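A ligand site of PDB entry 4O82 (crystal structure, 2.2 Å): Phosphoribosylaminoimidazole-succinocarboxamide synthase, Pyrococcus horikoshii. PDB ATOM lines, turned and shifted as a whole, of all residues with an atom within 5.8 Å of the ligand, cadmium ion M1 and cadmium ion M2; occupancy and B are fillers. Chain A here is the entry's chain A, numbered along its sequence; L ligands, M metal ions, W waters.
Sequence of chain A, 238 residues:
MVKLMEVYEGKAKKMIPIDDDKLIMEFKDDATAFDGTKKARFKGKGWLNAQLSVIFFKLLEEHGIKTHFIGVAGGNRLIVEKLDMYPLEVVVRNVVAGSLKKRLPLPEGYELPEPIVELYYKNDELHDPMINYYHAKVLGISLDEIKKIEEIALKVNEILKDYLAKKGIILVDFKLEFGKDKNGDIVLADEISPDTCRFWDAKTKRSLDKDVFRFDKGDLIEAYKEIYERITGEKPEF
Water W1 lies within hydrogen-bond range of an oxygen (O1) of the ligand (2.6 Å) and the side-chain hydroxyl (OH) of Tyr 120 (3.4 Å).
No residue comes within 4 Å of cadmium ion M2.
O of Asp 173 sits at hydrogen-bond distance from O6 of the ligand (3.5 Å).
An oxygen (O6) of the ligand sits at hydrogen-bond distance from the side-chain carboxylate of Asp 173.
An oxygen (O2) of the ligand is in salt-bridge range of the guanidinium group (NH2) of Arg 93, 2.8 Å away.
The backbone NH (N) of Arg 198 is in hydrogen-bond range of an oxygen (O6) of the ligand (3.3 Å).
The guanidinium group (NH1) of Arg 198 lies within salt-bridge range of an oxygen (O2) of the ligand (2.8 Å).
N of Ser 99 is in hydrogen-bond range of O2 of the ligand (2.9 Å).
OG of Ser 99 is in hydrogen-bond range of O1 of the ligand, at 2.9 Å.
Cadmium ion M1 is bound by OE1 of Glu 89 (2.2 Å) and N2 of the ligand (2.4 Å).
Cadmium ion M1 has two donor atoms within binding distance.
Of the 22 residues printed, 1 comes within 4 Å of cadmium ion M1.
The nearest printed residue that does not touch cadmium ion M1 is Asp 128 (4.1 Å).
N4 of the ligand binds cadmium ion M2.
Cadmium ion M2 is bound by water W2 (2.4 Å).
The backbone carbonyl oxygen of Glu 89 lies within hydrogen-bond range of the backbone NH of Tyr 120, 2.9 Å away.
The guanidinium group (NH1) of Arg 198 lies within salt-bridge range of the side-chain carboxylate (OD2) of Asp 173 (3.0 Å).
The guanidinium group (NH1) of Arg 93 is in hydrogen-bond range of the side-chain hydroxyl (OG) of Ser 99, at 3.4 Å.
The guanidinium group (NH2) of Arg 93 sits at hydrogen-bond distance from the backbone carbonyl oxygen (O) of Ala 97 (2.9 Å).
OE1 of Glu 118 is in salt-bridge range of NH1 of Arg 93 (2.8 Å).
O of Thr 196 sits at hydrogen-bond distance from N of Lys 175 (2.9 Å).
The side-chain carboxylate (OE2) of Glu 177 lies within salt-bridge range of the side-chain amino group (NZ) of Lys 175.
N of Glu 118 lies within hydrogen-bond range of O of Val 91, at 2.7 Å.
Val 91 touches the ligand.
Ala 97 touches the ligand.
Gly 98 touches the ligand.
CA of Phe 174 touches O6 of the ligand (3.6 Å).
CB of Lys 175 touches N1 of the ligand, at 3.6 Å.
Asp 195 touches the ligand (O to N5, 3.6 Å).
Thr 196 touches the ligand.
Cys 197 touches the ligand (C to O6, 3.4 Å).
NH1 of Arg 214 touches O7 of the ligand (3.6 Å).
Hydrophobic or aromatic side chains that line the ligand: Val 91.
14 residues have an atom within 4 Å of the ligand: Glu 89, Val 91, Arg 93, Ala 97, Gly 98, Ser 99, Asp 173, Phe 174, Lys 175, Asp 195, Thr 196, Cys 197, Arg 198 and Arg 214.
The nearest printed residue that does not touch the ligand is Tyr 120 (4.1 Å).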
ATOM      1  N   GLU A  89     -24.810  25.383 -37.936  1.00  0.00           N
ATOM      2  CA  GLU A  89     -24.851  24.398 -36.861  1.00  0.00           C
ATOM      3  C   GLU A  89     -26.257  24.421 -36.334  1.00  0.00           C
ATOM      4  O   GLU A  89     -26.757  25.481 -35.934  1.00  0.00           O
ATOM      5  CB  GLU A  89     -23.951  24.777 -35.698  1.00  0.00           C
ATOM      6  CG  GLU A  89     -22.482  24.841 -36.018  1.00  0.00           C
ATOM      7  CD  GLU A  89     -21.679  25.391 -34.855  1.00  0.00           C
ATOM      8  OE1 GLU A  89     -22.293  25.934 -33.898  1.00  0.00           O
ATOM      9  OE2 GLU A  89     -20.432  25.273 -34.907  1.00  0.00           O
ATOM     10  N   VAL A  91     -28.447  23.128 -33.433  1.00  0.00           N
ATOM     11  CA  VAL A  91     -28.304  22.611 -32.092  1.00  0.00           C
ATOM     12  C   VAL A  91     -29.661  22.276 -31.482  1.00  0.00           C
ATOM     13  O   VAL A  91     -30.571  23.095 -31.493  1.00  0.00           O
ATOM     14  CB  VAL A  91     -27.464  23.560 -31.191  1.00  0.00           C
ATOM     15  CG1 VAL A  91     -27.357  23.013 -29.773  1.00  0.00           C
ATOM     16  CG2 VAL A  91     -26.051  23.747 -31.763  1.00  0.00           C
ATOM     17  N   ARG A  93     -31.481  20.795 -27.884  1.00  0.00           N
ATOM     18  CA  ARG A  93     -31.192  20.805 -26.463  1.00  0.00           C
ATOM     19  C   ARG A  93     -32.382  20.280 -25.673  1.00  0.00           C
ATOM     20  O   ARG A  93     -33.497  20.802 -25.788  1.00  0.00           O
ATOM     21  CB  ARG A  93     -30.787  22.220 -25.977  1.00  0.00           C
ATOM     22  CG  ARG A  93     -29.874  22.954 -26.969  1.00  0.00           C
ATOM     23  CD  ARG A  93     -29.425  24.329 -26.485  1.00  0.00           C
ATOM     24  NE  ARG A  93     -28.310  24.177 -25.568  1.00  0.00           N
ATOM     25  CZ  ARG A  93     -27.106  24.707 -25.717  1.00  0.00           C
ATOM     26  NH1 ARG A  93     -26.811  25.497 -26.730  1.00  0.00           N
ATOM     27  NH2 ARG A  93     -26.189  24.472 -24.806  1.00  0.00           N
ATOM     28  N   ALA A  97     -27.451  23.104 -20.356  1.00  0.00           N
ATOM     29  CA  ALA A  97     -26.020  22.937 -20.197  1.00  0.00           C
ATOM     30  C   ALA A  97     -25.293  23.969 -21.059  1.00  0.00           C
ATOM     31  O   ALA A  97     -25.901  24.581 -21.942  1.00  0.00           O
ATOM     32  CB  ALA A  97     -25.611  21.512 -20.589  1.00  0.00           C
ATOM     33  N   GLY A  98     -23.998  24.151 -20.809  1.00  0.00           N
ATOM     34  CA  GLY A  98     -23.129  25.034 -21.620  1.00  0.00           C
ATOM     35  C   GLY A  98     -23.726  26.425 -21.774  1.00  0.00           C
ATOM     36  O   GLY A  98     -24.151  27.026 -20.779  1.00  0.00           O
ATOM     37  N   SER A  99     -23.821  26.891 -23.017  1.00  0.00           N
ATOM     38  CA  SER A  99     -24.170  28.268 -23.350  1.00  0.00           C
ATOM     39  C   SER A  99     -25.662  28.593 -23.134  1.00  0.00           C
ATOM     40  O   SER A  99     -26.030  29.779 -23.044  1.00  0.00           O
ATOM     41  CB  SER A  99     -23.790  28.589 -24.797  1.00  0.00           C
ATOM     42  OG  SER A  99     -24.714  28.009 -25.722  1.00  0.00           O
ATOM     43  N   LEU A 100     -26.513  27.563 -23.035  1.00  0.00           N
ATOM     44  CA  LEU A 100     -27.911  27.796 -22.724  1.00  0.00           C
ATOM     45  C   LEU A 100     -28.074  28.455 -21.337  1.00  0.00           C
ATOM     46  O   LEU A 100     -29.021  29.210 -21.110  1.00  0.00           O
ATOM     47  CB  LEU A 100     -28.702  26.490 -22.806  1.00  0.00           C
ATOM     48  CG  LEU A 100     -30.219  26.548 -22.639  1.00  0.00           C
ATOM     49  CD1 LEU A 100     -30.813  27.483 -23.675  1.00  0.00           C
ATOM     50  CD2 LEU A 100     -30.825  25.161 -22.760  1.00  0.00           C
ATOM     51  N   GLU A 118     -31.644  25.592 -31.695  1.00  0.00           N
ATOM     52  CA  GLU A 118     -30.947  26.834 -32.011  1.00  0.00           C
ATOM     53  C   GLU A 118     -30.178  26.676 -33.308  1.00  0.00           C
ATOM     54  O   GLU A 118     -29.629  25.598 -33.599  1.00  0.00           O
ATOM     55  CB  GLU A 118     -29.986  27.225 -30.899  1.00  0.00           C
ATOM     56  CG  GLU A 118     -30.630  27.298 -29.526  1.00  0.00           C
ATOM     57  CD  GLU A 118     -29.609  27.296 -28.401  1.00  0.00           C
ATOM     58  OE1 GLU A 118     -28.452  26.796 -28.593  1.00  0.00           O
ATOM     59  OE2 GLU A 118     -29.973  27.764 -27.304  1.00  0.00           O
ATOM     60  N   TYR A 120     -27.034  28.384 -35.548  1.00  0.00           N
ATOM     61  CA  TYR A 120     -25.841  29.165 -35.471  1.00  0.00           C
ATOM     62  C   TYR A 120     -25.268  29.272 -36.855  1.00  0.00           C
ATOM     63  O   TYR A 120     -25.303  28.301 -37.625  1.00  0.00           O
ATOM     64  CB  TYR A 120     -24.817  28.479 -34.591  1.00  0.00           C
ATOM     65  CG  TYR A 120     -25.184  28.445 -33.151  1.00  0.00           C
ATOM     66  CD1 TYR A 120     -24.706  29.421 -32.278  1.00  0.00           C
ATOM     67  CD2 TYR A 120     -26.054  27.449 -32.660  1.00  0.00           C
ATOM     68  CE1 TYR A 120     -25.067  29.385 -30.925  1.00  0.00           C
ATOM     69  CE2 TYR A 120     -26.412  27.421 -31.321  1.00  0.00           C
ATOM     70  CZ  TYR A 120     -25.907  28.373 -30.458  1.00  0.00           C
ATOM     71  OH  TYR A 120     -26.279  28.357 -29.162  1.00  0.00           O
ATOM     72  N   LYS A 122     -22.375  29.135 -39.284  1.00  0.00           N
ATOM     73  CA  LYS A 122     -21.064  28.492 -39.328  1.00  0.00           C
ATOM     74  C   LYS A 122     -20.051  29.463 -39.899  1.00  0.00           C
ATOM     75  O   LYS A 122     -20.064  29.748 -41.096  1.00  0.00           O
ATOM     76  CB  LYS A 122     -21.144  27.207 -40.141  1.00  0.00           C
ATOM     77  CG  LYS A 122     -20.322  26.056 -39.567  1.00  0.00           C
ATOM     78  CD  LYS A 122     -20.440  24.802 -40.436  1.00  0.00           C
ATOM     79  CE  LYS A 122     -19.166  23.978 -40.390  1.00  0.00           C
ATOM     80  NZ  LYS A 122     -18.812  23.599 -38.992  1.00  0.00           N
ATOM     81  N   ASP A 128     -19.041  31.503 -34.718  1.00  0.00           N
ATOM     82  CA  ASP A 128     -20.357  30.795 -34.799  1.00  0.00           C
ATOM     83  C   ASP A 128     -21.504  31.449 -34.020  1.00  0.00           C
ATOM     84  O   ASP A 128     -21.999  30.888 -33.056  1.00  0.00           O
ATOM     85  CB  ASP A 128     -20.233  29.318 -34.353  1.00  0.00           C
ATOM     86  CG  ASP A 128     -19.202  28.544 -35.167  1.00  0.00           C
ATOM     87  OD1 ASP A 128     -19.135  28.736 -36.410  1.00  0.00           O
ATOM     88  OD2 ASP A 128     -18.435  27.767 -34.570  1.00  0.00           O
ATOM     89  N   ASP A 173     -27.618  17.741 -25.126  1.00  0.00           N
ATOM     90  CA  ASP A 173     -27.751  18.578 -26.305  1.00  0.00           C
ATOM     91  C   ASP A 173     -26.809  17.988 -27.342  1.00  0.00           C
ATOM     92  O   ASP A 173     -26.024  17.061 -27.022  1.00  0.00           O
ATOM     93  CB  ASP A 173     -27.434  20.062 -26.006  1.00  0.00           C
ATOM     94  CG  ASP A 173     -26.096  20.249 -25.304  1.00  0.00           C
ATOM     95  OD1 ASP A 173     -25.088  19.711 -25.775  1.00  0.00           O
ATOM     96  OD2 ASP A 173     -26.054  20.922 -24.271  1.00  0.00           O
ATOM     97  N   PHE A 174     -26.911  18.490 -28.579  1.00  0.00           N
ATOM     98  CA  PHE A 174     -26.046  18.057 -29.661  1.00  0.00           C
ATOM     99  C   PHE A 174     -26.146  18.996 -30.872  1.00  0.00           C
ATOM    100  O   PHE A 174     -27.090  19.754 -30.975  1.00  0.00           O
ATOM    101  CB  PHE A 174     -26.304  16.583 -30.039  1.00  0.00           C
ATOM    102  CG  PHE A 174     -27.642  16.321 -30.643  1.00  0.00           C
ATOM    103  CD1 PHE A 174     -27.752  16.008 -31.985  1.00  0.00           C
ATOM    104  CD2 PHE A 174     -28.794  16.345 -29.875  1.00  0.00           C
ATOM    105  CE1 PHE A 174     -28.993  15.752 -32.573  1.00  0.00           C
ATOM    106  CE2 PHE A 174     -30.030  16.119 -30.458  1.00  0.00           C
ATOM    107  CZ  PHE A 174     -30.132  15.825 -31.803  1.00  0.00           C
ATOM    108  N   LYS A 175     -25.145  18.933 -31.761  1.00  0.00           N
ATOM    109  CA  LYS A 175     -25.067  19.792 -32.938  1.00  0.00           C
ATOM    110  C   LYS A 175     -25.155  18.947 -34.196  1.00  0.00           C
ATOM    111  O   LYS A 175     -24.507  17.930 -34.282  1.00  0.00           O
ATOM    112  CB  LYS A 175     -23.768  20.612 -32.984  1.00  0.00           C
ATOM    113  CG  LYS A 175     -23.563  21.381 -34.292  1.00  0.00           C
ATOM    114  CD  LYS A 175     -22.146  21.380 -34.872  1.00  0.00           C
ATOM    115  CE  LYS A 175     -21.450  20.031 -34.926  1.00  0.00           C
ATOM    116  NZ  LYS A 175     -20.758  19.818 -36.216  1.00  0.00           N
ATOM    117  N   GLU A 177     -25.341  19.088 -38.697  1.00  0.00           N
ATOM    118  CA  GLU A 177     -25.124  19.810 -39.910  1.00  0.00           C
ATOM    119  C   GLU A 177     -25.891  19.098 -41.030  1.00  0.00           C
ATOM    120  O   GLU A 177     -26.105  17.867 -40.952  1.00  0.00           O
ATOM    121  CB  GLU A 177     -23.623  19.913 -40.236  1.00  0.00           C
ATOM    122  CG  GLU A 177     -22.816  20.433 -39.043  1.00  0.00           C
ATOM    123  CD  GLU A 177     -21.398  20.852 -39.382  1.00  0.00           C
ATOM    124  OE1 GLU A 177     -20.995  20.880 -40.569  1.00  0.00           O
ATOM    125  OE2 GLU A 177     -20.673  21.192 -38.423  1.00  0.00           O
ATOM    126  N   PRO A 194     -19.379  11.712 -29.434  1.00  0.00           N
ATOM    127  CA  PRO A 194     -19.213  12.449 -28.178  1.00  0.00           C
ATOM    128  C   PRO A 194     -18.437  13.760 -28.373  1.00  0.00           C
ATOM    129  O   PRO A 194     -18.316  14.532 -27.428  1.00  0.00           O
ATOM    130  CB  PRO A 194     -18.408  11.484 -27.301  1.00  0.00           C
ATOM    131  CG  PRO A 194     -18.544  10.135 -27.932  1.00  0.00           C
ATOM    132  CD  PRO A 194     -18.721  10.401 -29.400  1.00  0.00           C
ATOM    133  N   ASP A 195     -17.906  14.018 -29.563  1.00  0.00           N
ATOM    134  CA  ASP A 195     -17.364  15.319 -29.914  1.00  0.00           C
ATOM    135  C   ASP A 195     -18.456  16.381 -30.163  1.00  0.00           C
ATOM    136  O   ASP A 195     -18.239  17.578 -29.960  1.00  0.00           O
ATOM    137  CB  ASP A 195     -16.464  15.202 -31.144  1.00  0.00           C
ATOM    138  CG  ASP A 195     -15.039  14.764 -30.809  1.00  0.00           C
ATOM    139  OD1 ASP A 195     -14.152  14.915 -31.663  1.00  0.00           O
ATOM    140  OD2 ASP A 195     -14.803  14.292 -29.683  1.00  0.00           O
ATOM    141  N   THR A 196     -19.617  15.923 -30.617  1.00  0.00           N
ATOM    142  CA  THR A 196     -20.662  16.831 -31.082  1.00  0.00           C
ATOM    143  C   THR A 196     -21.990  16.731 -30.313  1.00  0.00           C
ATOM    144  O   THR A 196     -22.981  17.319 -30.719  1.00  0.00           O
ATOM    145  CB  THR A 196     -20.932  16.609 -32.569  1.00  0.00           C
ATOM    146  OG1 THR A 196     -21.367  15.275 -32.757  1.00  0.00           O
ATOM    147  CG2 THR A 196     -19.641  16.870 -33.395  1.00  0.00           C
ATOM    148  N   CYS A 197     -21.983  15.980 -29.211  1.00  0.00           N
ATOM    149  CA  CYS A 197     -23.130  15.856 -28.298  1.00  0.00           C
ATOM    150  C   CYS A 197     -22.657  15.933 -26.861  1.00  0.00           C
ATOM    151  O   CYS A 197     -21.505  15.603 -26.565  1.00  0.00           O
ATOM    152  CB  CYS A 197     -23.829  14.486 -28.415  1.00  0.00           C
ATOM    153  SG  CYS A 197     -23.996  13.757 -30.057  1.00  0.00           S
ATOM    154  N   ARG A 198     -23.553  16.333 -25.973  1.00  0.00           N
ATOM    155  CA  ARG A 198     -23.347  16.148 -24.557  1.00  0.00           C
ATOM    156  C   ARG A 198     -24.138  14.928 -24.110  1.00  0.00           C
ATOM    157  O   ARG A 198     -25.386  14.890 -24.176  1.00  0.00           O
ATOM    158  CB  ARG A 198     -23.741  17.388 -23.747  1.00  0.00           C
ATOM    159  CG  ARG A 198     -22.791  18.570 -23.875  1.00  0.00           C
ATOM    160  CD  ARG A 198     -23.039  19.641 -22.792  1.00  0.00           C
ATOM    161  NE  ARG A 198     -22.032  20.708 -22.869  1.00  0.00           N
ATOM    162  CZ  ARG A 198     -22.193  21.857 -23.545  1.00  0.00           C
ATOM    163  NH1 ARG A 198     -23.334  22.141 -24.183  1.00  0.00           N
ATOM    164  NH2 ARG A 198     -21.209  22.733 -23.570  1.00  0.00           N
ATOM    165  N   LYS A 210     -16.863  15.243 -24.971  1.00  0.00           N
ATOM    166  CA  LYS A 210     -15.736  16.147 -25.087  1.00  0.00           C
ATOM    167  C   LYS A 210     -15.581  17.130 -23.904  1.00  0.00           C
ATOM    168  O   LYS A 210     -14.521  17.725 -23.740  1.00  0.00           O
ATOM    169  CB  LYS A 210     -15.801  16.905 -26.418  1.00  0.00           C
ATOM    170  CG  LYS A 210     -14.477  17.477 -26.892  1.00  0.00           C
ATOM    171  CD  LYS A 210     -14.579  17.919 -28.353  1.00  0.00           C
ATOM    172  CE  LYS A 210     -13.632  19.079 -28.672  1.00  0.00           C
ATOM    173  NZ  LYS A 210     -13.671  19.431 -30.128  1.00  0.00           N
ATOM    174  N   ARG A 214     -12.581  19.395 -22.489  1.00  0.00           N
ATOM    175  CA  ARG A 214     -12.704  20.857 -22.427  1.00  0.00           C
ATOM    176  C   ARG A 214     -12.397  21.409 -21.054  1.00  0.00           C
ATOM    177  O   ARG A 214     -11.772  22.453 -20.905  1.00  0.00           O
ATOM    178  CB  ARG A 214     -14.111  21.313 -22.823  1.00  0.00           C
ATOM    179  CG  ARG A 214     -14.408  21.245 -24.303  1.00  0.00           C
ATOM    180  CD  ARG A 214     -15.733  21.916 -24.624  1.00  0.00           C
ATOM    181  NE  ARG A 214     -16.173  21.532 -25.958  1.00  0.00           N
ATOM    182  CZ  ARG A 214     -17.071  20.597 -26.224  1.00  0.00           C
ATOM    183  NH1 ARG A 214     -17.393  20.328 -27.480  1.00  0.00           N
ATOM    184  NH2 ARG A 214     -17.667  19.939 -25.241  1.00  0.00           N
HETATM  185  P1  LIG L   1     -22.883  24.937 -26.435  1.00  0.00           P
HETATM  186  O1  LIG L   1     -23.605  25.920 -27.338  1.00  0.00           O
HETATM  187  O2  LIG L   1     -23.424  24.841 -25.020  1.00  0.00           O
HETATM  188  O3  LIG L   1     -21.378  25.020 -26.382  1.00  0.00           O
HETATM  189  O4  LIG L   1     -23.082  23.529 -27.233  1.00  0.00           O
HETATM  190  C1  LIG L   1     -24.301  22.788 -27.438  1.00  0.00           C
HETATM  191  C2  LIG L   1     -24.047  21.411 -28.057  1.00  0.00           C
HETATM  192  O5  LIG L   1     -23.649  21.538 -29.422  1.00  0.00           O
HETATM  193  C3  LIG L   1     -22.938  20.562 -27.426  1.00  0.00           C
HETATM  194  O6  LIG L   1     -23.332  19.199 -27.531  1.00  0.00           O
HETATM  195  C4  LIG L   1     -21.727  20.752 -28.294  1.00  0.00           C
HETATM  196  O7  LIG L   1     -20.831  19.624 -28.267  1.00  0.00           O
HETATM  197  C5  LIG L   1     -22.370  20.950 -29.658  1.00  0.00           C
HETATM  198  N1  LIG L   1     -21.566  21.867 -30.492  1.00  0.00           N
HETATM  199  C6  LIG L   1     -21.775  23.188 -30.632  1.00  0.00           C
HETATM  200  N2  LIG L   1     -20.873  23.724 -31.494  1.00  0.00           N
HETATM  201  C7  LIG L   1     -20.074  22.735 -31.914  1.00  0.00           C
HETATM  202  C8  LIG L   1     -18.908  22.611 -32.827  1.00  0.00           C
HETATM  203  N3  LIG L   1     -18.407  23.698 -33.472  1.00  0.00           N
HETATM  204  N4  LIG L   1     -18.383  21.374 -32.989  1.00  0.00           N
HETATM  205  C9  LIG L   1     -18.863  20.287 -32.368  1.00  0.00           C
HETATM  206  N5  LIG L   1     -19.914  20.333 -31.521  1.00  0.00           N
HETATM  207  C10 LIG L   1     -20.542  21.504 -31.263  1.00  0.00           C
HETATM  208 CD    CD M   1     -21.124  26.090 -32.045  1.00  0.00          CD
HETATM  209 CD    CD M   2     -16.528  21.046 -34.513  1.00  0.00          CD
HETATM  210 CD    CD M   3     -16.621  20.303 -37.542  1.00  0.00          CD
HETATM  211 CD    CD M   4     -17.276  26.676 -36.127  1.00  0.00          CD
HETATM  212  O   HOH W   1     -22.930  27.688 -29.131  1.00  0.00           O
HETATM  213  O   HOH W   2     -14.698  19.923 -35.665  1.00  0.00           O
HETATM  214  O   HOH W   3     -19.204  17.576 -26.885  1.00  0.00           O
